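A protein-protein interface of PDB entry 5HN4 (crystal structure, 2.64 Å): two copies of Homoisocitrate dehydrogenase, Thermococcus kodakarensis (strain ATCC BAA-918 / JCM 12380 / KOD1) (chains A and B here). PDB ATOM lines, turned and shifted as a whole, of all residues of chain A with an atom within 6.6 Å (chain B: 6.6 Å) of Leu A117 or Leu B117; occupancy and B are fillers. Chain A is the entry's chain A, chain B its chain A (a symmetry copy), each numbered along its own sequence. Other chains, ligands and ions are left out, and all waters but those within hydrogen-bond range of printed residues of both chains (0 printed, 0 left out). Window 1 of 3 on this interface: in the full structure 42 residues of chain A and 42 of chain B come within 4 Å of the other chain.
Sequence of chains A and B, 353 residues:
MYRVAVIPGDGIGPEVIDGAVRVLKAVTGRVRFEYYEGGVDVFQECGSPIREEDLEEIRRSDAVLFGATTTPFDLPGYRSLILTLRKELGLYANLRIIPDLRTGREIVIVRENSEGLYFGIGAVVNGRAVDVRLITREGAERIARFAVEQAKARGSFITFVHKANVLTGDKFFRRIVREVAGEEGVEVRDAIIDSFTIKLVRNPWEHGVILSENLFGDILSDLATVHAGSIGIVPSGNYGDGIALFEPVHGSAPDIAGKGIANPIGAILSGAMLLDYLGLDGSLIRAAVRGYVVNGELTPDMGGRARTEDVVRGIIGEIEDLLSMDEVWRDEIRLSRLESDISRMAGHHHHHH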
ATOM      1  N   GLU A 115      -7.458  29.157  -3.180  1.00  0.00           N
ATOM      2  CA  GLU A 115      -8.518  28.852  -4.152  1.00  0.00           C
ATOM      3  C   GLU A 115      -9.850  28.499  -3.477  1.00  0.00           C
ATOM      4  O   GLU A 115     -10.251  29.182  -2.529  1.00  0.00           O
ATOM      5  CB  GLU A 115      -8.041  27.833  -5.190  1.00  0.00           C
ATOM      6  CG  GLU A 115      -7.458  26.554  -4.633  1.00  0.00           C
ATOM      7  CD  GLU A 115      -6.823  25.651  -5.700  1.00  0.00           C
ATOM      8  OE1 GLU A 115      -6.906  24.418  -5.502  1.00  0.00           O
ATOM      9  OE2 GLU A 115      -6.237  26.147  -6.715  1.00  0.00           O
ATOM     10  N   GLY A 116     -10.558  27.491  -3.974  1.00  0.00           N
ATOM     11  CA  GLY A 116     -11.828  27.131  -3.415  1.00  0.00           C
ATOM     12  C   GLY A 116     -12.810  28.220  -3.724  1.00  0.00           C
ATOM     13  O   GLY A 116     -12.823  28.717  -4.792  1.00  0.00           O
ATOM     14  N   LEU A 117     -13.633  28.602  -2.770  1.00  0.00           N
ATOM     15  CA  LEU A 117     -14.643  29.603  -3.028  1.00  0.00           C
ATOM     16  C   LEU A 117     -14.058  30.988  -2.991  1.00  0.00           C
ATOM     17  O   LEU A 117     -14.755  31.958  -3.267  1.00  0.00           O
ATOM     18  CB  LEU A 117     -15.828  29.434  -2.042  1.00  0.00           C
ATOM     19  CG  LEU A 117     -16.900  28.474  -2.621  1.00  0.00           C
ATOM     20  CD1 LEU A 117     -17.907  28.033  -1.598  1.00  0.00           C
ATOM     21  CD2 LEU A 117     -17.619  29.118  -3.811  1.00  0.00           C
ATOM     22  N   TYR A 118     -12.782  31.088  -2.638  1.00  0.00           N
ATOM     23  CA  TYR A 118     -12.058  32.366  -2.618  1.00  0.00           C
ATOM     24  C   TYR A 118     -11.387  32.647  -3.960  1.00  0.00           C
ATOM     25  O   TYR A 118     -10.823  33.719  -4.141  1.00  0.00           O
ATOM     26  CB  TYR A 118     -10.969  32.379  -1.500  1.00  0.00           C
ATOM     27  CG  TYR A 118     -11.503  32.616  -0.112  1.00  0.00           C
ATOM     28  CD1 TYR A 118     -12.194  31.609   0.581  1.00  0.00           C
ATOM     29  CD2 TYR A 118     -11.348  33.856   0.504  1.00  0.00           C
ATOM     30  CE1 TYR A 118     -12.706  31.839   1.837  1.00  0.00           C
ATOM     31  CE2 TYR A 118     -11.851  34.094   1.763  1.00  0.00           C
ATOM     32  CZ  TYR A 118     -12.532  33.094   2.421  1.00  0.00           C
ATOM     33  OH  TYR A 118     -12.984  33.349   3.682  1.00  0.00           O
ATOM     34  N   PHE A 119     -11.408  31.701  -4.896  1.00  0.00           N
ATOM     35  CA  PHE A 119     -10.712  31.931  -6.175  1.00  0.00           C
ATOM     36  C   PHE A 119     -11.080  33.241  -6.866  1.00  0.00           C
ATOM     37  O   PHE A 119     -10.243  33.856  -7.486  1.00  0.00           O
ATOM     38  CB  PHE A 119     -10.872  30.780  -7.168  1.00  0.00           C
ATOM     39  CG  PHE A 119      -9.916  30.874  -8.335  1.00  0.00           C
ATOM     40  CD1 PHE A 119      -8.526  30.859  -8.119  1.00  0.00           C
ATOM     41  CD2 PHE A 119     -10.385  31.008  -9.638  1.00  0.00           C
ATOM     42  CE1 PHE A 119      -7.635  30.952  -9.181  1.00  0.00           C
ATOM     43  CE2 PHE A 119      -9.497  31.103 -10.699  1.00  0.00           C
ATOM     44  CZ  PHE A 119      -8.124  31.074 -10.471  1.00  0.00           C
ATOM     45  N   GLY A 120     -12.326  33.651  -6.746  1.00  0.00           N
ATOM     46  CA  GLY A 120     -12.730  34.963  -7.173  1.00  0.00           C
ATOM     47  C   GLY A 120     -13.619  35.028  -8.397  1.00  0.00           C
ATOM     48  O   GLY A 120     -13.984  36.104  -8.802  1.00  0.00           O
ATOM     49  N   ILE A 121     -13.973  33.899  -8.989  1.00  0.00           N
ATOM     50  CA  ILE A 121     -14.880  33.904 -10.131  1.00  0.00           C
ATOM     51  C   ILE A 121     -16.345  33.923  -9.748  1.00  0.00           C
ATOM     52  O   ILE A 121     -16.895  32.896  -9.352  1.00  0.00           O
ATOM     53  CB  ILE A 121     -14.656  32.701 -11.033  1.00  0.00           C
ATOM     54  CG1 ILE A 121     -13.188  32.650 -11.464  1.00  0.00           C
ATOM     55  CG2 ILE A 121     -15.608  32.780 -12.232  1.00  0.00           C
ATOM     56  CD1 ILE A 121     -12.762  31.288 -11.974  1.00  0.00           C
ATOM     57  N   ASP A 131     -21.047  31.557  -7.908  1.00  0.00           N
ATOM     58  CA  ASP A 131     -19.655  31.603  -7.436  1.00  0.00           C
ATOM     59  C   ASP A 131     -19.094  30.243  -7.744  1.00  0.00           C
ATOM     60  O   ASP A 131     -19.788  29.248  -7.553  1.00  0.00           O
ATOM     61  CB  ASP A 131     -19.529  31.866  -5.937  1.00  0.00           C
ATOM     62  CG  ASP A 131     -19.819  33.327  -5.537  1.00  0.00           C
ATOM     63  OD1 ASP A 131     -18.902  34.169  -5.584  1.00  0.00           O
ATOM     64  OD2 ASP A 131     -20.946  33.642  -5.139  1.00  0.00           O
ATOM     65  N   VAL A 132     -17.832  30.200  -8.172  1.00  0.00           N
ATOM     66  CA  VAL A 132     -17.195  28.996  -8.640  1.00  0.00           C
ATOM     67  C   VAL A 132     -16.185  28.525  -7.592  1.00  0.00           C
ATOM     68  O   VAL A 132     -15.204  29.201  -7.345  1.00  0.00           O
ATOM     69  CB  VAL A 132     -16.477  29.254 -10.003  1.00  0.00           C
ATOM     70  CG1 VAL A 132     -15.774  28.003 -10.508  1.00  0.00           C
ATOM     71  CG2 VAL A 132     -17.466  29.770 -11.051  1.00  0.00           C
ATOM     72  N   ARG A 133     -16.447  27.361  -6.992  1.00  0.00           N
ATOM     73  CA  ARG A 133     -15.554  26.717  -6.045  1.00  0.00           C
ATOM     74  C   ARG A 133     -14.532  25.951  -6.873  1.00  0.00           C
ATOM     75  O   ARG A 133     -14.845  24.906  -7.422  1.00  0.00           O
ATOM     76  CB  ARG A 133     -16.344  25.767  -5.078  1.00  0.00           C
ATOM     77  CG  ARG A 133     -15.574  25.397  -3.806  1.00  0.00           C
ATOM     78  CD  ARG A 133     -16.323  24.519  -2.767  1.00  0.00           C
ATOM     79  NE  ARG A 133     -15.720  23.216  -2.863  1.00  0.00           N
ATOM     80  CZ  ARG A 133     -15.085  22.515  -1.944  1.00  0.00           C
ATOM     81  NH1 ARG A 133     -14.980  22.853  -0.692  1.00  0.00           N
ATOM     82  NH2 ARG A 133     -14.601  21.367  -2.323  1.00  0.00           N
ATOM     83  N   LEU A 134     -13.310  26.476  -6.962  1.00  0.00           N
ATOM     84  CA  LEU A 134     -12.264  25.908  -7.805  1.00  0.00           C
ATOM     85  C   LEU A 134     -11.223  25.201  -6.998  1.00  0.00           C
ATOM     86  O   LEU A 134     -10.667  25.775  -6.088  1.00  0.00           O
ATOM     87  CB  LEU A 134     -11.571  26.988  -8.612  1.00  0.00           C
ATOM     88  CG  LEU A 134     -10.314  26.577  -9.387  1.00  0.00           C
ATOM     89  CD1 LEU A 134     -10.647  25.678 -10.565  1.00  0.00           C
ATOM     90  CD2 LEU A 134      -9.566  27.792  -9.891  1.00  0.00           C
ATOM     91  N   ILE A 135     -10.950  23.948  -7.349  1.00  0.00           N
ATOM     92  CA  ILE A 135      -9.823  23.208  -6.814  1.00  0.00           C
ATOM     93  C   ILE A 135      -8.921  22.846  -7.981  1.00  0.00           C
ATOM     94  O   ILE A 135      -9.413  22.320  -8.959  1.00  0.00           O
ATOM     95  CB  ILE A 135     -10.300  21.903  -6.195  1.00  0.00           C
ATOM     96  CG1 ILE A 135     -11.457  22.151  -5.232  1.00  0.00           C
ATOM     97  CG2 ILE A 135      -9.153  21.187  -5.514  1.00  0.00           C
ATOM     98  CD1 ILE A 135     -11.136  23.047  -4.057  1.00  0.00           C
ATOM     99  N   VAL A 166     -21.324  15.714  -2.588  1.00  0.00           N
ATOM    100  CA  VAL A 166     -22.019  16.798  -3.246  1.00  0.00           C
ATOM    101  C   VAL A 166     -21.085  17.588  -4.128  1.00  0.00           C
ATOM    102  O   VAL A 166     -21.546  18.167  -5.110  1.00  0.00           O
ATOM    103  CB  VAL A 166     -22.659  17.732  -2.197  1.00  0.00           C
ATOM    104  CG1 VAL A 166     -23.362  18.927  -2.811  1.00  0.00           C
ATOM    105  CG2 VAL A 166     -23.662  16.980  -1.355  1.00  0.00           C
ATOM    106  N   LEU A 167     -19.790  17.618  -3.812  1.00  0.00           N
ATOM    107  CA  LEU A 167     -18.860  18.505  -4.500  1.00  0.00           C
ATOM    108  C   LEU A 167     -17.807  17.772  -5.347  1.00  0.00           C
ATOM    109  O   LEU A 167     -16.940  17.058  -4.844  1.00  0.00           O
ATOM    110  CB  LEU A 167     -18.154  19.385  -3.463  1.00  0.00           C
ATOM    111  CG  LEU A 167     -19.062  20.209  -2.545  1.00  0.00           C
ATOM    112  CD1 LEU A 167     -18.245  21.009  -1.533  1.00  0.00           C
ATOM    113  CD2 LEU A 167     -19.942  21.122  -3.380  1.00  0.00           C
ATOM    114  N   GLU A 213     -10.616  22.680   2.341  1.00  0.00           N
ATOM    115  CA  GLU A 213     -10.738  23.777   1.371  1.00  0.00           C
ATOM    116  C   GLU A 213     -10.892  25.104   2.112  1.00  0.00           C
ATOM    117  O   GLU A 213     -11.288  25.140   3.268  1.00  0.00           O
ATOM    118  CB  GLU A 213     -11.946  23.525   0.460  1.00  0.00           C
ATOM    119  CG  GLU A 213     -12.352  24.612  -0.503  1.00  0.00           C
ATOM    120  CD  GLU A 213     -13.191  25.712   0.131  1.00  0.00           C
ATOM    121  OE1 GLU A 213     -13.141  26.831  -0.392  1.00  0.00           O
ATOM    122  OE2 GLU A 213     -13.909  25.475   1.120  1.00  0.00           O
ATOM    123  N   ASN A 214     -10.589  26.178   1.410  1.00  0.00           N
ATOM    124  CA  ASN A 214     -10.476  27.503   1.965  1.00  0.00           C
ATOM    125  C   ASN A 214     -11.638  27.954   2.844  1.00  0.00           C
ATOM    126  O   ASN A 214     -11.431  28.269   4.029  1.00  0.00           O
ATOM    127  CB  ASN A 214     -10.284  28.473   0.815  1.00  0.00           C
ATOM    128  CG  ASN A 214      -9.621  29.758   1.221  1.00  0.00           C
ATOM    129  OD1 ASN A 214      -9.828  30.283   2.307  1.00  0.00           O
ATOM    130  ND2 ASN A 214      -8.854  30.302   0.315  1.00  0.00           N
ATOM    131  N   LEU A 215     -12.841  28.006   2.285  1.00  0.00           N
ATOM    132  CA  LEU A 215     -13.989  28.488   3.034  1.00  0.00           C
ATOM    133  C   LEU A 215     -14.317  27.522   4.176  1.00  0.00           C
ATOM    134  O   LEU A 215     -14.592  27.970   5.284  1.00  0.00           O
ATOM    135  CB  LEU A 215     -15.205  28.686   2.132  1.00  0.00           C
ATOM    136  CG  LEU A 215     -16.406  29.293   2.841  1.00  0.00           C
ATOM    137  CD1 LEU A 215     -16.115  30.667   3.395  1.00  0.00           C
ATOM    138  CD2 LEU A 215     -17.579  29.340   1.895  1.00  0.00           C
ATOM    139  N   PHE A 216     -14.282  26.213   3.923  1.00  0.00           N
ATOM    140  CA  PHE A 216     -14.467  25.253   5.007  1.00  0.00           C
ATOM    141  C   PHE A 216     -13.470  25.510   6.130  1.00  0.00           C
ATOM    142  O   PHE A 216     -13.812  25.408   7.298  1.00  0.00           O
ATOM    143  CB  PHE A 216     -14.315  23.818   4.538  1.00  0.00           C
ATOM    144  CG  PHE A 216     -15.456  23.303   3.700  1.00  0.00           C
ATOM    145  CD1 PHE A 216     -16.707  23.913   3.686  1.00  0.00           C
ATOM    146  CD2 PHE A 216     -15.288  22.150   2.949  1.00  0.00           C
ATOM    147  CE1 PHE A 216     -17.733  23.418   2.880  1.00  0.00           C
ATOM    148  CE2 PHE A 216     -16.299  21.654   2.170  1.00  0.00           C
ATOM    149  CZ  PHE A 216     -17.524  22.287   2.128  1.00  0.00           C
ATOM    150  N   GLU B 115     -30.863  24.796  -4.114  1.00  0.00           N
ATOM    151  CA  GLU B 115     -29.773  25.328  -4.946  1.00  0.00           C
ATOM    152  C   GLU B 115     -28.465  25.498  -4.162  1.00  0.00           C
ATOM    153  O   GLU B 115     -28.093  24.600  -3.399  1.00  0.00           O
ATOM    154  CB  GLU B 115     -30.220  26.574  -5.715  1.00  0.00           C
ATOM    155  CG  GLU B 115     -30.826  27.677  -4.879  1.00  0.00           C
ATOM    156  CD  GLU B 115     -31.429  28.819  -5.710  1.00  0.00           C
ATOM    157  OE1 GLU B 115     -31.358  29.964  -5.211  1.00  0.00           O
ATOM    158  OE2 GLU B 115     -31.980  28.591  -6.834  1.00  0.00           O
ATOM    159  N   GLY B 116     -27.745  26.594  -4.371  1.00  0.00           N
ATOM    160  CA  GLY B 116     -26.496  26.799  -3.699  1.00  0.00           C
ATOM    161  C   GLY B 116     -25.500  25.816  -4.235  1.00  0.00           C
ATOM    162  O   GLY B 116     -25.451  25.598  -5.392  1.00  0.00           O
ATOM    163  N   LEU B 117     -24.707  25.207  -3.379  1.00  0.00           N
ATOM    164  CA  LEU B 117     -23.685  24.298  -3.843  1.00  0.00           C
ATOM    165  C   LEU B 117     -24.265  22.948  -4.168  1.00  0.00           C
ATOM    166  O   LEU B 117     -23.555  22.074  -4.652  1.00  0.00           O
ATOM    167  CB  LEU B 117     -22.534  24.213  -2.808  1.00  0.00           C
ATOM    168  CG  LEU B 117     -21.447  25.281  -3.097  1.00  0.00           C
ATOM    169  CD1 LEU B 117     -20.475  25.453  -1.964  1.00  0.00           C
ATOM    170  CD2 LEU B 117     -20.688  24.949  -4.384  1.00  0.00           C
ATOM    171  N   TYR B 118     -25.552  22.770  -3.892  1.00  0.00           N
ATOM    172  CA  TYR B 118     -26.271  21.529  -4.213  1.00  0.00           C
ATOM    173  C   TYR B 118     -26.897  21.591  -5.603  1.00  0.00           C
ATOM    174  O   TYR B 118     -27.450  20.599  -6.061  1.00  0.00           O
ATOM    175  CB  TYR B 118     -27.395  21.245  -3.168  1.00  0.00           C
ATOM    176  CG  TYR B 118     -26.906  20.670  -1.865  1.00  0.00           C
ATOM    177  CD1 TYR B 118     -26.242  21.473  -0.923  1.00  0.00           C
ATOM    178  CD2 TYR B 118     -27.076  19.318  -1.579  1.00  0.00           C
ATOM    179  CE1 TYR B 118     -25.771  20.938   0.254  1.00  0.00           C
ATOM    180  CE2 TYR B 118     -26.614  18.775  -0.403  1.00  0.00           C
ATOM    181  CZ  TYR B 118     -25.958  19.578   0.504  1.00  0.00           C
ATOM    182  OH  TYR B 118     -25.546  19.017   1.677  1.00  0.00           O
ATOM    183  N   PHE B 119     -26.849  22.739  -6.276  1.00  0.00           N
ATOM    184  CA  PHE B 119     -27.502  22.834  -7.593  1.00  0.00           C
ATOM    185  C   PHE B 119     -27.106  21.734  -8.574  1.00  0.00           C
ATOM    186  O   PHE B 119     -27.921  21.294  -9.354  1.00  0.00           O
ATOM    187  CB  PHE B 119     -27.314  24.194  -8.265  1.00  0.00           C
ATOM    188  CG  PHE B 119     -28.232  24.395  -9.451  1.00  0.00           C
ATOM    189  CD1 PHE B 119     -29.627  24.362  -9.283  1.00  0.00           C
ATOM    190  CD2 PHE B 119     -27.720  24.585 -10.730  1.00  0.00           C
ATOM    191  CE1 PHE B 119     -30.483  24.538 -10.363  1.00  0.00           C
ATOM    192  CE2 PHE B 119     -28.572  24.759 -11.811  1.00  0.00           C
ATOM    193  CZ  PHE B 119     -29.952  24.736 -11.627  1.00  0.00           C
ATOM    194  N   GLY B 120     -25.863  21.302  -8.518  1.00  0.00           N
ATOM    195  CA  GLY B 120     -25.440  20.134  -9.243  1.00  0.00           C
ATOM    196  C   GLY B 120     -24.511  20.369 -10.415  1.00  0.00           C
ATOM    197  O   GLY B 120     -24.129  19.425 -11.061  1.00  0.00           O
ATOM    198  N   ILE B 121     -24.143  21.608 -10.698  1.00  0.00           N
ATOM    199  CA  ILE B 121     -23.199  21.881 -11.776  1.00  0.00           C
ATOM    200  C   ILE B 121     -21.748  21.762 -11.363  1.00  0.00           C
ATOM    201  O   ILE B 121     -21.215  22.658 -10.708  1.00  0.00           O
ATOM    202  CB  ILE B 121     -23.398  23.271 -12.360  1.00  0.00           C
ATOM    203  CG1 ILE B 121     -24.852  23.432 -12.813  1.00  0.00           C
ATOM    204  CG2 ILE B 121     -22.408  23.486 -13.510  1.00  0.00           C
ATOM    205  CD1 ILE B 121     -25.267  24.881 -12.984  1.00  0.00           C
ATOM    206  N   ASP B 131     -17.117  23.582  -8.843  1.00  0.00           N
ATOM    207  CA  ASP B 131     -18.524  23.426  -8.442  1.00  0.00           C
ATOM    208  C   ASP B 131     -19.080  24.823  -8.424  1.00  0.00           C
ATOM    209  O   ASP B 131     -18.397  25.737  -7.971  1.00  0.00           O
ATOM    210  CB  ASP B 131     -18.698  22.803  -7.059  1.00  0.00           C
ATOM    211  CG  ASP B 131     -18.415  21.287  -7.024  1.00  0.00           C
ATOM    212  OD1 ASP B 131     -19.327  20.487  -7.307  1.00  0.00           O
ATOM    213  OD2 ASP B 131     -17.301  20.879  -6.679  1.00  0.00           O
ATOM    214  N   VAL B 132     -20.328  24.975  -8.869  1.00  0.00           N
ATOM    215  CA  VAL B 132     -20.954  26.260  -9.045  1.00  0.00           C
ATOM    216  C   VAL B 132     -22.000  26.463  -7.947  1.00  0.00           C
ATOM    217  O   VAL B 132     -22.985  25.750  -7.906  1.00  0.00           O
ATOM    218  CB  VAL B 132     -21.626  26.350 -10.452  1.00  0.00           C
ATOM    219  CG1 VAL B 132     -22.318  27.689 -10.655  1.00  0.00           C
ATOM    220  CG2 VAL B 132     -20.601  26.105 -11.563  1.00  0.00           C
ATOM    221  N   ARG B 133     -21.762  27.441  -7.070  1.00  0.00           N
ATOM    222  CA  ARG B 133     -22.688  27.835  -6.023  1.00  0.00           C
ATOM    223  C   ARG B 133     -23.685  28.785  -6.670  1.00  0.00           C
ATOM    224  O   ARG B 133     -23.359  29.932  -6.932  1.00  0.00           O
ATOM    225  CB  ARG B 133     -21.934  28.514  -4.826  1.00  0.00           C
ATOM    226  CG  ARG B 133     -22.747  28.561  -3.528  1.00  0.00           C
ATOM    227  CD  ARG B 133     -22.035  29.153  -2.281  1.00  0.00           C
ATOM    228  NE  ARG B 133     -22.640  30.442  -2.072  1.00  0.00           N
ATOM    229  CZ  ARG B 133     -23.307  30.896  -1.030  1.00  0.00           C
ATOM    230  NH1 ARG B 133     -23.452  30.260   0.097  1.00  0.00           N
ATOM    231  NH2 ARG B 133     -23.784  32.104  -1.129  1.00  0.00           N
ATOM    232  N   LEU B 134     -24.902  28.304  -6.925  1.00  0.00           N
ATOM    233  CA  LEU B 134     -25.923  29.067  -7.635  1.00  0.00           C
ATOM    234  C   LEU B 134     -26.992  29.556  -6.712  1.00  0.00           C
ATOM    235  O   LEU B 134     -27.575  28.778  -5.991  1.00  0.00           O
ATOM    236  CB  LEU B 134     -26.584  28.222  -8.706  1.00  0.00           C
ATOM    237  CG  LEU B 134     -27.817  28.817  -9.395  1.00  0.00           C
ATOM    238  CD1 LEU B 134     -27.450  29.977 -10.304  1.00  0.00           C
ATOM    239  CD2 LEU B 134     -28.544  27.767 -10.208  1.00  0.00           C
ATOM    240  N   ILE B 135     -27.258  30.859  -6.752  1.00  0.00           N
ATOM    241  CA  ILE B 135     -28.405  31.448  -6.089  1.00  0.00           C
ATOM    242  C   ILE B 135     -29.271  32.092  -7.159  1.00  0.00           C
ATOM    243  O   ILE B 135     -28.749  32.841  -7.960  1.00  0.00           O
ATOM    244  CB  ILE B 135     -27.954  32.559  -5.151  1.00  0.00           C
ATOM    245  CG1 ILE B 135     -26.828  32.075  -4.242  1.00  0.00           C
ATOM    246  CG2 ILE B 135     -29.125  33.089  -4.352  1.00  0.00           C
ATOM    247  CD1 ILE B 135     -27.183  30.918  -3.335  1.00  0.00           C
ATOM    248  N   VAL B 166     -17.079  37.621   0.229  1.00  0.00           N
ATOM    249  CA  VAL B 166     -16.358  36.730  -0.654  1.00  0.00           C
ATOM    250  C   VAL B 166     -17.259  36.186  -1.733  1.00  0.00           C
ATOM    251  O   VAL B 166     -16.765  35.865  -2.812  1.00  0.00           O
ATOM    252  CB  VAL B 166     -15.749  35.563   0.153  1.00  0.00           C
ATOM    253  CG1 VAL B 166     -15.022  34.554  -0.714  1.00  0.00           C
ATOM    254  CG2 VAL B 166     -14.777  36.080   1.187  1.00  0.00           C
ATOM    255  N   LEU B 167     -18.564  36.083  -1.476  1.00  0.00           N
ATOM    256  CA  LEU B 167     -19.468  35.398  -2.392  1.00  0.00           C
ATOM    257  C   LEU B 167     -20.495  36.322  -3.066  1.00  0.00           C
ATOM    258  O   LEU B 167     -21.381  36.893  -2.430  1.00  0.00           O
ATOM    259  CB  LEU B 167     -20.204  34.292  -1.628  1.00  0.00           C
ATOM    260  CG  LEU B 167     -19.323  33.264  -0.913  1.00  0.00           C
ATOM    261  CD1 LEU B 167     -20.169  32.242  -0.156  1.00  0.00           C
ATOM    262  CD2 LEU B 167     -18.412  32.581  -1.918  1.00  0.00           C
ATOM    263  N   GLU B 213     -27.913  29.697   2.935  1.00  0.00           N
ATOM    264  CA  GLU B 213     -27.755  28.873   1.728  1.00  0.00           C
ATOM    265  C   GLU B 213     -27.620  27.404   2.123  1.00  0.00           C
ATOM    266  O   GLU B 213     -27.262  27.082   3.247  1.00  0.00           O
ATOM    267  CB  GLU B 213     -26.519  29.337   0.948  1.00  0.00           C
ATOM    268  CG  GLU B 213     -26.078  28.520  -0.240  1.00  0.00           C
ATOM    269  CD  GLU B 213     -25.255  27.294   0.129  1.00  0.00           C
ATOM    270  OE1 GLU B 213     -25.283  26.339  -0.654  1.00  0.00           O
ATOM    271  OE2 GLU B 213     -24.570  27.277   1.169  1.00  0.00           O
ATOM    272  N   ASN B 214     -27.896  26.537   1.169  1.00  0.00           N
ATOM    273  CA  ASN B 214     -28.021  25.117   1.375  1.00  0.00           C
ATOM    274  C   ASN B 214     -26.887  24.459   2.153  1.00  0.00           C
ATOM    275  O   ASN B 214     -27.131  23.861   3.217  1.00  0.00           O
ATOM    276  CB  ASN B 214     -28.171  24.462   0.016  1.00  0.00           C
ATOM    277  CG  ASN B 214     -28.842  23.119   0.070  1.00  0.00           C
ATOM    278  OD1 ASN B 214     -28.669  22.341   0.999  1.00  0.00           O
ATOM    279  ND2 ASN B 214     -29.577  22.818  -0.966  1.00  0.00           N
ATOM    280  N   LEU B 215     -25.665  24.541   1.638  1.00  0.00           N
ATOM    281  CA  LEU B 215     -24.541  23.884   2.282  1.00  0.00           C
ATOM    282  C   LEU B 215     -24.254  24.537   3.637  1.00  0.00           C
ATOM    283  O   LEU B 215     -24.014  23.828   4.608  1.00  0.00           O
ATOM    284  CB  LEU B 215     -23.296  23.910   1.400  1.00  0.00           C
ATOM    285  CG  LEU B 215     -22.115  23.142   1.975  1.00  0.00           C
ATOM    286  CD1 LEU B 215     -22.419  21.674   2.163  1.00  0.00           C
ATOM    287  CD2 LEU B 215     -20.912  23.326   1.086  1.00  0.00           C
ATOM    288  N   PHE B 216     -24.286  25.868   3.714  1.00  0.00           N
ATOM    289  CA  PHE B 216     -24.141  26.530   5.007  1.00  0.00           C
ATOM    290  C   PHE B 216     -25.172  26.008   5.999  1.00  0.00           C
ATOM    291  O   PHE B 216     -24.869  25.817   7.166  1.00  0.00           O
ATOM    292  CB  PHE B 216     -24.283  28.038   4.902  1.00  0.00           C
ATOM    293  CG  PHE B 216     -23.117  28.738   4.255  1.00  0.00           C
ATOM    294  CD1 PHE B 216     -21.864  28.146   4.131  1.00  0.00           C
ATOM    295  CD2 PHE B 216     -23.266  30.042   3.807  1.00  0.00           C
ATOM    296  CE1 PHE B 216     -20.814  28.820   3.507  1.00  0.00           C
ATOM    297  CE2 PHE B 216     -22.232  30.711   3.207  1.00  0.00           C
ATOM    298  CZ  PHE B 216     -21.004  30.102   3.050  1.00  0.00           C
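Tyr A118 touches Val B166, and with the chains exchanged Val A166 touches Tyr B118.
Asp A131 touches Val B132, and with the chains exchanged Val A132 touches Asp B131.
Asp A131 touches Leu B167, and with the chains exchanged Leu A167 touches Asp B131.
Leu A215 touches Phe B216, and with the chains exchanged Phe A216 touches Leu B215.
18 positions are printed for both chains.
The backbone carbonyl oxygen (O) of Asp B131 lies within hydrogen-bond range of the backbone NH (N) of Arg A133 (2.7 Å).
The backbone carbonyl oxygen of Asp A131 lies within hydrogen-bond range of the backbone NH of Arg B133 (2.7 Å).
Leu A117 touches Leu B117.
O of Leu A117 touches CD2 of Leu B167 (3.9 Å).
Asp A131 touches Asp B131.
CA of Val B132 touches O of Asp A131, 3.5 Å away.
OD2 of Asp A131 touches C of Leu B167, at 3.4 Å.
Val A132 touches Asp B131.
Leu B117 touches Val A166.
CG2 of Val A166 touches CE2 of Tyr B118 (3.6 Å).
O of Leu B117 touches CD2 of Leu A167, at 3.9 Å.
Leu A215 touches Phe B216 (CD2 to CE1, 3.7 Å).
Leu A117 touches just these residues of chain B: Leu B117 (3.7 Å), Val B166 (3.7 Å) and Leu B167 (3.9 Å).
Leu B117 touches just these residues of chain A: Leu A117, Val A166 and Leu A167.
Printed residues of chain A within 4 Å of Asp B131: Asp A131, Val A132, Arg A133, Val A166 and Leu A167.
Printed residues of chain A within 4 Å of Val B132: Asp A131 (3.5 Å).
Leu A134 touches none of the printed residues of chain B.
Gly A120 touches none of the printed residues of chain B.
The nearest residue of chain B that does not touch Leu A117 is Arg B133 (4.3 Å).
The guanidinium group (NH1) of Arg A133 lies within salt-bridge range of the side-chain carboxylate (OE2) of Glu A213.
The side-chain carboxylate (OE2) of Glu A213 is in hydrogen-bond range of the backbone NH (N) of Phe A216.
The side-chain carboxylate (OE2) of Glu B213 is in salt-bridge range of the guanidinium group (NH1) of Arg B133 (3.4 Å).
The side-chain carboxylate (OE2) of Glu B213 is in hydrogen-bond range of the backbone NH (N) of Phe B216, at 2.9 Å.
OE1 of Glu A213 is in hydrogen-bond range of N of Leu A215 (2.9 Å).
The backbone carbonyl oxygen (O) of Ile A121 sits at hydrogen-bond distance from the backbone NH (N) of Val A132 (3.1 Å).
Hydrophobic or aromatic side chains of chain A within 4 Å of the printed part of chain B: Leu A117, Tyr A118, Val A166, Leu A167, Leu A215 and Phe A216.
Of the 18 printed residues of chain B, 9 touch a printed residue of chain A.
Hydrophobic or aromatic side chains of chain B that line the printed part of chain A: Leu B117, Tyr B118, Val B166, Leu B167, Leu B215 and Phe B216.
Among the printed residues, 18 pairs touch across the chains.
Among the printed residues, no Asp or Glu carboxylate lies within 4 Å of a Lys or Arg side-chain nitrogen of the other chain.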
